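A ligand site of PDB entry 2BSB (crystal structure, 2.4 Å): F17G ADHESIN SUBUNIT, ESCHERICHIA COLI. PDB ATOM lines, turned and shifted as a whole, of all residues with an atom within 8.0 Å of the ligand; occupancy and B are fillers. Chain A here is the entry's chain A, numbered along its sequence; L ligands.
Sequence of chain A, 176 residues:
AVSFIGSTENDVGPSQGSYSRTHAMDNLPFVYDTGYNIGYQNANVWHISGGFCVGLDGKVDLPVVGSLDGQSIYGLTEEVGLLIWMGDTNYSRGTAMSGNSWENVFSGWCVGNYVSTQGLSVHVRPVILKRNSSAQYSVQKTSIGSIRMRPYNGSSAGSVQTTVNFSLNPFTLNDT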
ATOM      1  N   ASN A  42      26.799  13.697  25.239  1.00  0.00           N
ATOM      2  CA  ASN A  42      27.787  12.886  24.550  1.00  0.00           C
ATOM      3  C   ASN A  42      27.829  13.347  23.117  1.00  0.00           C
ATOM      4  O   ASN A  42      26.842  13.246  22.388  1.00  0.00           O
ATOM      5  CB  ASN A  42      27.386  11.414  24.546  1.00  0.00           C
ATOM      6  CG  ASN A  42      28.502  10.508  24.011  1.00  0.00           C
ATOM      7  OD1 ASN A  42      29.296  10.915  23.165  1.00  0.00           O
ATOM      8  ND2 ASN A  42      28.536   9.273  24.498  1.00  0.00           N
ATOM      9  N   ALA A  43      28.992  13.832  22.710  1.00  0.00           N
ATOM     10  CA  ALA A  43      29.213  14.344  21.366  1.00  0.00           C
ATOM     11  C   ALA A  43      29.554  13.259  20.350  1.00  0.00           C
ATOM     12  O   ALA A  43      29.656  13.536  19.153  1.00  0.00           O
ATOM     13  CB  ALA A  43      30.304  15.379  21.405  1.00  0.00           C
ATOM     14  N   ASN A  44      29.721  12.034  20.809  1.00  0.00           N
ATOM     15  CA  ASN A  44      30.071  10.958  19.902  1.00  0.00           C
ATOM     16  C   ASN A  44      29.196   9.730  20.093  1.00  0.00           C
ATOM     17  O   ASN A  44      29.579   8.774  20.773  1.00  0.00           O
ATOM     18  CB  ASN A  44      31.530  10.571  20.081  1.00  0.00           C
ATOM     19  CG  ASN A  44      32.420  11.778  20.237  1.00  0.00           C
ATOM     20  OD1 ASN A  44      32.585  12.558  19.313  1.00  0.00           O
ATOM     21  ND2 ASN A  44      32.979  11.946  21.416  1.00  0.00           N
ATOM     22  N   VAL A  45      28.022   9.745  19.465  1.00  0.00           N
ATOM     23  CA  VAL A  45      27.091   8.634  19.547  1.00  0.00           C
ATOM     24  C   VAL A  45      27.045   7.912  18.214  1.00  0.00           C
ATOM     25  O   VAL A  45      26.744   6.718  18.133  1.00  0.00           O
ATOM     26  CB  VAL A  45      25.667   9.113  19.905  1.00  0.00           C
ATOM     27  CG1 VAL A  45      24.667   7.976  19.784  1.00  0.00           C
ATOM     28  CG2 VAL A  45      25.674   9.657  21.325  1.00  0.00           C
ATOM     29  N   TRP A  46      27.355   8.664  17.168  1.00  0.00           N
ATOM     30  CA  TRP A  46      27.386   8.124  15.827  1.00  0.00           C
ATOM     31  C   TRP A  46      28.645   8.599  15.149  1.00  0.00           C
ATOM     32  O   TRP A  46      29.162   9.685  15.440  1.00  0.00           O
ATOM     33  CB  TRP A  46      26.169   8.577  15.034  1.00  0.00           C
ATOM     34  CG  TRP A  46      24.930   7.845  15.364  1.00  0.00           C
ATOM     35  CD1 TRP A  46      24.592   6.581  14.974  1.00  0.00           C
ATOM     36  CD2 TRP A  46      23.856   8.322  16.193  1.00  0.00           C
ATOM     37  NE1 TRP A  46      23.368   6.237  15.515  1.00  0.00           N
ATOM     38  CE2 TRP A  46      22.893   7.282  16.259  1.00  0.00           C
ATOM     39  CE3 TRP A  46      23.616   9.510  16.884  1.00  0.00           C
ATOM     40  CZ2 TRP A  46      21.718   7.405  16.995  1.00  0.00           C
ATOM     41  CZ3 TRP A  46      22.444   9.632  17.606  1.00  0.00           C
ATOM     42  CH2 TRP A  46      21.507   8.588  17.655  1.00  0.00           C
ATOM     43  N   ILE A  48      29.989   9.473  11.498  1.00  0.00           N
ATOM     44  CA  ILE A  48      29.518   9.781  10.150  1.00  0.00           C
ATOM     45  C   ILE A  48      30.634  10.262   9.219  1.00  0.00           C
ATOM     46  O   ILE A  48      31.611  10.869   9.669  1.00  0.00           O
ATOM     47  CB  ILE A  48      28.402  10.829  10.153  1.00  0.00           C
ATOM     48  CG1 ILE A  48      28.886  12.109  10.835  1.00  0.00           C
ATOM     49  CG2 ILE A  48      27.158  10.260  10.834  1.00  0.00           C
ATOM     50  CD1 ILE A  48      27.877  13.204  10.871  1.00  0.00           C
ATOM     51  N   VAL A  54      22.614  13.968   8.798  1.00  0.00           N
ATOM     52  CA  VAL A  54      21.820  13.417   9.885  1.00  0.00           C
ATOM     53  C   VAL A  54      21.283  14.475  10.849  1.00  0.00           C
ATOM     54  O   VAL A  54      21.914  15.507  11.067  1.00  0.00           O
ATOM     55  CB  VAL A  54      22.629  12.382  10.669  1.00  0.00           C
ATOM     56  CG1 VAL A  54      23.805  13.065  11.368  1.00  0.00           C
ATOM     57  CG2 VAL A  54      21.736  11.667  11.648  1.00  0.00           C
ATOM     58  N   LEU A  56      18.121  14.855  14.394  1.00  0.00           N
ATOM     59  CA  LEU A  56      17.683  14.110  15.576  1.00  0.00           C
ATOM     60  C   LEU A  56      16.196  14.239  15.920  1.00  0.00           C
ATOM     61  O   LEU A  56      15.607  15.309  15.781  1.00  0.00           O
ATOM     62  CB  LEU A  56      18.516  14.532  16.800  1.00  0.00           C
ATOM     63  CG  LEU A  56      20.039  14.351  16.819  1.00  0.00           C
ATOM     64  CD1 LEU A  56      20.608  14.995  18.070  1.00  0.00           C
ATOM     65  CD2 LEU A  56      20.379  12.862  16.791  1.00  0.00           C
ATOM     66  N   GLY A  87      18.132  17.430  22.203  1.00  0.00           N
ATOM     67  CA  GLY A  87      18.661  18.058  21.012  1.00  0.00           C
ATOM     68  C   GLY A  87      20.094  17.672  20.743  1.00  0.00           C
ATOM     69  O   GLY A  87      20.575  16.652  21.247  1.00  0.00           O
ATOM     70  N   ASP A  88      20.786  18.511  19.962  1.00  0.00           N
ATOM     71  CA  ASP A  88      22.166  18.295  19.605  1.00  0.00           C
ATOM     72  C   ASP A  88      23.118  18.385  20.817  1.00  0.00           C
ATOM     73  O   ASP A  88      22.723  18.816  21.906  1.00  0.00           O
ATOM     74  CB  ASP A  88      22.598  19.273  18.508  1.00  0.00           C
ATOM     75  CG  ASP A  88      23.900  18.878  17.853  1.00  0.00           C
ATOM     76  OD1 ASP A  88      24.211  17.665  17.848  1.00  0.00           O
ATOM     77  OD2 ASP A  88      24.611  19.768  17.337  1.00  0.00           O
ATOM     78  N   THR A  89      24.369  17.990  20.581  1.00  0.00           N
ATOM     79  CA  THR A  89      25.422  17.932  21.595  1.00  0.00           C
ATOM     80  C   THR A  89      25.448  19.063  22.604  1.00  0.00           C
ATOM     81  O   THR A  89      25.314  18.818  23.805  1.00  0.00           O
ATOM     82  CB  THR A  89      26.800  17.784  20.921  1.00  0.00           C
ATOM     83  OG1 THR A  89      26.842  16.559  20.186  1.00  0.00           O
ATOM     84  CG2 THR A  89      27.913  17.775  21.973  1.00  0.00           C
ATOM     85  N   ASN A  90      25.633  20.283  22.137  1.00  0.00           N
ATOM     86  CA  ASN A  90      25.654  21.430  23.034  1.00  0.00           C
ATOM     87  C   ASN A  90      24.309  21.581  23.750  1.00  0.00           C
ATOM     88  O   ASN A  90      23.240  21.532  23.114  1.00  0.00           O
ATOM     89  CB  ASN A  90      25.955  22.705  22.244  1.00  0.00           C
ATOM     90  CG  ASN A  90      27.283  22.622  21.515  1.00  0.00           C
ATOM     91  OD1 ASN A  90      28.346  22.622  22.143  1.00  0.00           O
ATOM     92  ND2 ASN A  90      27.231  22.546  20.194  1.00  0.00           N
ATOM     93  N   ARG A  93      21.558  24.194  22.801  1.00  0.00           N
ATOM     94  CA  ARG A  93      20.906  23.945  21.516  1.00  0.00           C
ATOM     95  C   ARG A  93      19.835  22.874  21.618  1.00  0.00           C
ATOM     96  O   ARG A  93      19.651  22.075  20.701  1.00  0.00           O
ATOM     97  CB  ARG A  93      21.962  23.546  20.482  1.00  0.00           C
ATOM     98  CG  ARG A  93      22.186  24.603  19.416  1.00  0.00           C
ATOM     99  CD  ARG A  93      23.565  24.510  18.777  1.00  0.00           C
ATOM    100  NE  ARG A  93      24.602  25.145  19.597  1.00  0.00           N
ATOM    101  CZ  ARG A  93      25.852  25.344  19.201  1.00  0.00           C
ATOM    102  NH1 ARG A  93      26.732  25.928  20.022  1.00  0.00           N
ATOM    103  NH2 ARG A  93      26.242  24.961  17.994  1.00  0.00           N
ATOM    104  N   PHE A 106      16.535  18.439  16.452  1.00  0.00           N
ATOM    105  CA  PHE A 106      17.711  19.022  15.822  1.00  0.00           C
ATOM    106  C   PHE A 106      17.538  18.845  14.321  1.00  0.00           C
ATOM    107  O   PHE A 106      17.482  17.721  13.821  1.00  0.00           O
ATOM    108  CB  PHE A 106      18.986  18.306  16.311  1.00  0.00           C
ATOM    109  CG  PHE A 106      20.227  18.679  15.529  1.00  0.00           C
ATOM    110  CD1 PHE A 106      20.586  20.004  15.339  1.00  0.00           C
ATOM    111  CD2 PHE A 106      21.063  17.679  15.010  1.00  0.00           C
ATOM    112  CE1 PHE A 106      21.764  20.358  14.650  1.00  0.00           C
ATOM    113  CE2 PHE A 106      22.244  18.011  14.319  1.00  0.00           C
ATOM    114  CZ  PHE A 106      22.595  19.366  14.129  1.00  0.00           C
ATOM    115  N   GLY A 108      19.489  18.963  12.005  1.00  0.00           N
ATOM    116  CA  GLY A 108      20.594  18.260  11.349  1.00  0.00           C
ATOM    117  C   GLY A 108      21.614  19.011  10.504  1.00  0.00           C
ATOM    118  O   GLY A 108      21.492  20.202  10.234  1.00  0.00           O
ATOM    119  N   TRP A 109      22.638  18.268  10.072  1.00  0.00           N
ATOM    120  CA  TRP A 109      23.726  18.797   9.252  1.00  0.00           C
ATOM    121  C   TRP A 109      24.278  17.708   8.362  1.00  0.00           C
ATOM    122  O   TRP A 109      23.879  16.546   8.461  1.00  0.00           O
ATOM    123  CB  TRP A 109      24.851  19.334  10.148  1.00  0.00           C
ATOM    124  CG  TRP A 109      25.686  18.267  10.839  1.00  0.00           C
ATOM    125  CD1 TRP A 109      25.241  17.300  11.685  1.00  0.00           C
ATOM    126  CD2 TRP A 109      27.113  18.108  10.765  1.00  0.00           C
ATOM    127  NE1 TRP A 109      26.294  16.541  12.148  1.00  0.00           N
ATOM    128  CE2 TRP A 109      27.449  17.009  11.597  1.00  0.00           C
ATOM    129  CE3 TRP A 109      28.153  18.771  10.075  1.00  0.00           C
ATOM    130  CZ2 TRP A 109      28.783  16.572  11.769  1.00  0.00           C
ATOM    131  CZ3 TRP A 109      29.474  18.327  10.246  1.00  0.00           C
ATOM    132  CH2 TRP A 109      29.771  17.225  11.094  1.00  0.00           C
ATOM    133  N   CYS A 110      25.221  18.076   7.491  1.00  0.00           N
ATOM    134  CA  CYS A 110      25.849  17.123   6.593  1.00  0.00           C
ATOM    135  C   CYS A 110      27.365  17.243   6.701  1.00  0.00           C
ATOM    136  O   CYS A 110      27.918  18.317   6.455  1.00  0.00           O
ATOM    137  CB  CYS A 110      25.453  17.384   5.142  1.00  0.00           C
ATOM    138  SG  CYS A 110      23.677  17.432   4.742  1.00  0.00           S
ATOM    139  N   VAL A 111      28.034  16.147   7.040  1.00  0.00           N
ATOM    140  CA  VAL A 111      29.482  16.147   7.156  1.00  0.00           C
ATOM    141  C   VAL A 111      30.039  16.156   5.749  1.00  0.00           C
ATOM    142  O   VAL A 111      29.396  15.660   4.825  1.00  0.00           O
ATOM    143  CB  VAL A 111      30.003  14.887   7.901  1.00  0.00           C
ATOM    144  CG1 VAL A 111      29.625  13.616   7.142  1.00  0.00           C
ATOM    145  CG2 VAL A 111      31.498  14.975   8.055  1.00  0.00           C
ATOM    146  N   TYR A 114      34.760  13.830   4.941  1.00  0.00           N
ATOM    147  CA  TYR A 114      35.648  13.465   6.039  1.00  0.00           C
ATOM    148  C   TYR A 114      34.929  12.763   7.200  1.00  0.00           C
ATOM    149  O   TYR A 114      33.712  12.628   7.192  1.00  0.00           O
ATOM    150  CB  TYR A 114      36.387  14.712   6.555  1.00  0.00           C
ATOM    151  CG  TYR A 114      35.490  15.801   7.092  1.00  0.00           C
ATOM    152  CD1 TYR A 114      34.990  15.747   8.393  1.00  0.00           C
ATOM    153  CD2 TYR A 114      35.133  16.887   6.294  1.00  0.00           C
ATOM    154  CE1 TYR A 114      34.160  16.756   8.889  1.00  0.00           C
ATOM    155  CE2 TYR A 114      34.305  17.894   6.777  1.00  0.00           C
ATOM    156  CZ  TYR A 114      33.821  17.824   8.076  1.00  0.00           C
ATOM    157  OH  TYR A 114      33.009  18.816   8.557  1.00  0.00           O
ATOM    158  N   VAL A 115      35.704  12.329   8.187  1.00  0.00           N
ATOM    159  CA  VAL A 115      35.164  11.619   9.338  1.00  0.00           C
ATOM    160  C   VAL A 115      34.889  12.539  10.523  1.00  0.00           C
ATOM    161  O   VAL A 115      35.780  13.234  10.994  1.00  0.00           O
ATOM    162  CB  VAL A 115      36.134  10.530   9.817  1.00  0.00           C
ATOM    163  CG1 VAL A 115      35.455   9.688  10.884  1.00  0.00           C
ATOM    164  CG2 VAL A 115      36.594   9.681   8.654  1.00  0.00           C
ATOM    165  N   SER A 116      33.644  12.507  10.995  1.00  0.00           N
ATOM    166  CA  SER A 116      33.185  13.308  12.145  1.00  0.00           C
ATOM    167  C   SER A 116      32.189  12.469  12.958  1.00  0.00           C
ATOM    168  O   SER A 116      32.137  11.250  12.801  1.00  0.00           O
ATOM    169  CB  SER A 116      32.515  14.594  11.659  1.00  0.00           C
ATOM    170  OG  SER A 116      32.060  15.402  12.735  1.00  0.00           O
ATOM    171  N   THR A 117      31.404  13.110  13.805  1.00  0.00           N
ATOM    172  CA  THR A 117      30.428  12.386  14.632  1.00  0.00           C
ATOM    173  C   THR A 117      29.143  13.179  14.892  1.00  0.00           C
ATOM    174  O   THR A 117      29.061  14.382  14.642  1.00  0.00           O
ATOM    175  CB  THR A 117      31.014  12.010  16.034  1.00  0.00           C
ATOM    176  OG1 THR A 117      31.092  13.186  16.849  1.00  0.00           O
ATOM    177  CG2 THR A 117      32.404  11.411  15.900  1.00  0.00           C
ATOM    178  N   GLN A 118      28.141  12.472  15.421  1.00  0.00           N
ATOM    179  CA  GLN A 118      26.870  13.076  15.765  1.00  0.00           C
ATOM    180  C   GLN A 118      26.619  12.774  17.237  1.00  0.00           C
ATOM    181  O   GLN A 118      26.655  11.613  17.655  1.00  0.00           O
ATOM    182  CB  GLN A 118      25.759  12.487  14.903  1.00  0.00           C
ATOM    183  CG  GLN A 118      24.377  13.009  15.262  1.00  0.00           C
ATOM    184  CD  GLN A 118      24.298  14.514  15.225  1.00  0.00           C
ATOM    185  OE1 GLN A 118      24.688  15.153  14.255  1.00  0.00           O
ATOM    186  NE2 GLN A 118      23.773  15.096  16.303  1.00  0.00           N
ATOM    187  N   GLY A 119      26.382  13.827  18.016  1.00  0.00           N
ATOM    188  CA  GLY A 119      26.147  13.664  19.425  1.00  0.00           C
ATOM    189  C   GLY A 119      24.755  14.125  19.784  1.00  0.00           C
ATOM    190  O   GLY A 119      23.912  14.385  18.915  1.00  0.00           O
ATOM    191  N   LEU A 120      24.518  14.242  21.090  1.00  0.00           N
ATOM    192  CA  LEU A 120      23.223  14.657  21.584  1.00  0.00           C
ATOM    193  C   LEU A 120      23.394  15.090  23.022  1.00  0.00           C
ATOM    194  O   LEU A 120      24.462  14.913  23.613  1.00  0.00           O
ATOM    195  CB  LEU A 120      22.253  13.470  21.482  1.00  0.00           C
ATOM    196  CG  LEU A 120      22.732  12.138  22.058  1.00  0.00           C
ATOM    197  CD1 LEU A 120      22.798  12.257  23.571  1.00  0.00           C
ATOM    198  CD2 LEU A 120      21.778  11.044  21.654  1.00  0.00           C
ATOM    199  N   SER A 121      22.328  15.652  23.584  1.00  0.00           N
ATOM    200  CA  SER A 121      22.317  16.111  24.970  1.00  0.00           C
ATOM    201  C   SER A 121      20.885  16.020  25.469  1.00  0.00           C
ATOM    202  O   SER A 121      19.941  16.051  24.690  1.00  0.00           O
ATOM    203  CB  SER A 121      22.834  17.551  25.088  1.00  0.00           C
ATOM    204  OG  SER A 121      21.933  18.513  24.554  1.00  0.00           O
HETATM  205  C1  LIG L   1      29.972  17.681  15.203  1.00  0.00           C
HETATM  206  C2  LIG L   1      30.089  17.144  16.626  1.00  0.00           C
HETATM  207  C3  LIG L   1      28.820  16.393  17.027  1.00  0.00           C
HETATM  208  C4  LIG L   1      27.570  17.254  16.758  1.00  0.00           C
HETATM  209  C5  LIG L   1      27.597  17.716  15.308  1.00  0.00           C
HETATM  210  C6  LIG L   1      26.409  18.574  14.906  1.00  0.00           C
HETATM  211  C7  LIG L   1      32.179  16.448  17.659  1.00  0.00           C
HETATM  212  C8  LIG L   1      32.531  17.882  18.024  1.00  0.00           C
HETATM  213  N1  LIG L   1      31.229  16.248  16.734  1.00  0.00           N
HETATM  214  O1  LIG L   1      31.060  18.481  14.936  1.00  0.00           O
HETATM  215  O2  LIG L   1      28.895  16.075  18.407  1.00  0.00           O
HETATM  216  O3  LIG L   1      26.398  16.486  16.997  1.00  0.00           O
HETATM  217  O4  LIG L   1      28.794  18.483  15.066  1.00  0.00           O
HETATM  218  O5  LIG L   1      26.430  19.833  15.567  1.00  0.00           O
HETATM  219  O6  LIG L   1      32.782  15.513  18.178  1.00  0.00           O
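The side-chain amide oxygen of Asn 44 is in hydrogen-bond range of the side-chain hydroxyl of Thr 117, 2.9 Å away. The backbone carbonyl oxygen (O) of Asp 88 lies within hydrogen-bond range of the side-chain hydroxyl (OG) of Ser 121, 2.8 Å away. The side-chain hydroxyl (OG1) of Thr 89 lies within hydrogen-bond range of the backbone NH (N) of Leu 120 (3.4 Å). The backbone carbonyl oxygen (O) of Trp 46 is in hydrogen-bond range of the backbone NH (N) of Gln 118. O of Thr 89 lies close to OG of Ser 121 (3.5 Å). O of Phe 106 is in hydrogen-bond range of N of Leu 56, at 3.0 Å. O of Trp 109 sits at hydrogen-bond distance from N of Val 54, 2.9 Å away. The side-chain carboxylate (OD1) of Asp 88 sits at hydrogen-bond distance from the side-chain amide nitrogen (NE2) of Gln 118 (3.0 Å).
O5 of the ligand lies within hydrogen-bond range of OD2 of Asp 88 (2.5 Å). The backbone carbonyl oxygen of Ala 43 is in hydrogen-bond range of an oxygen (O2) of the ligand (2.8 Å). O3 of the ligand sits at hydrogen-bond distance from N of Gly 119, 2.8 Å away. The side-chain hydroxyl (OG1) of Thr 117 is in hydrogen-bond range of a nitrogen (N1) of the ligand, 3.1 Å away. NE2 of Gln 118 sits at hydrogen-bond distance from O3 of the ligand (3.1 Å). The side-chain hydroxyl (OG1) of Thr 89 is in hydrogen-bond range of an oxygen (O2) of the ligand (2.8 Å). The side-chain amide oxygen of Asn 44 lies close to an oxygen (O6) of the ligand, 3.2 Å away.
Phe 106 touches the ligand. NE1 of Trp 109 touches C6 of the ligand, 3.4 Å away. OG of Ser 116 touches O1 of the ligand (3.9 Å). Hydrophobic or aromatic side chains within 4 Å of the ligand: Ala 43, Phe 106 and Trp 109. Of the 26 residues printed, 10 come within 4 Å of the ligand. The nearest printed residue that does not touch the ligand is Leu 120 (5.0 Å).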
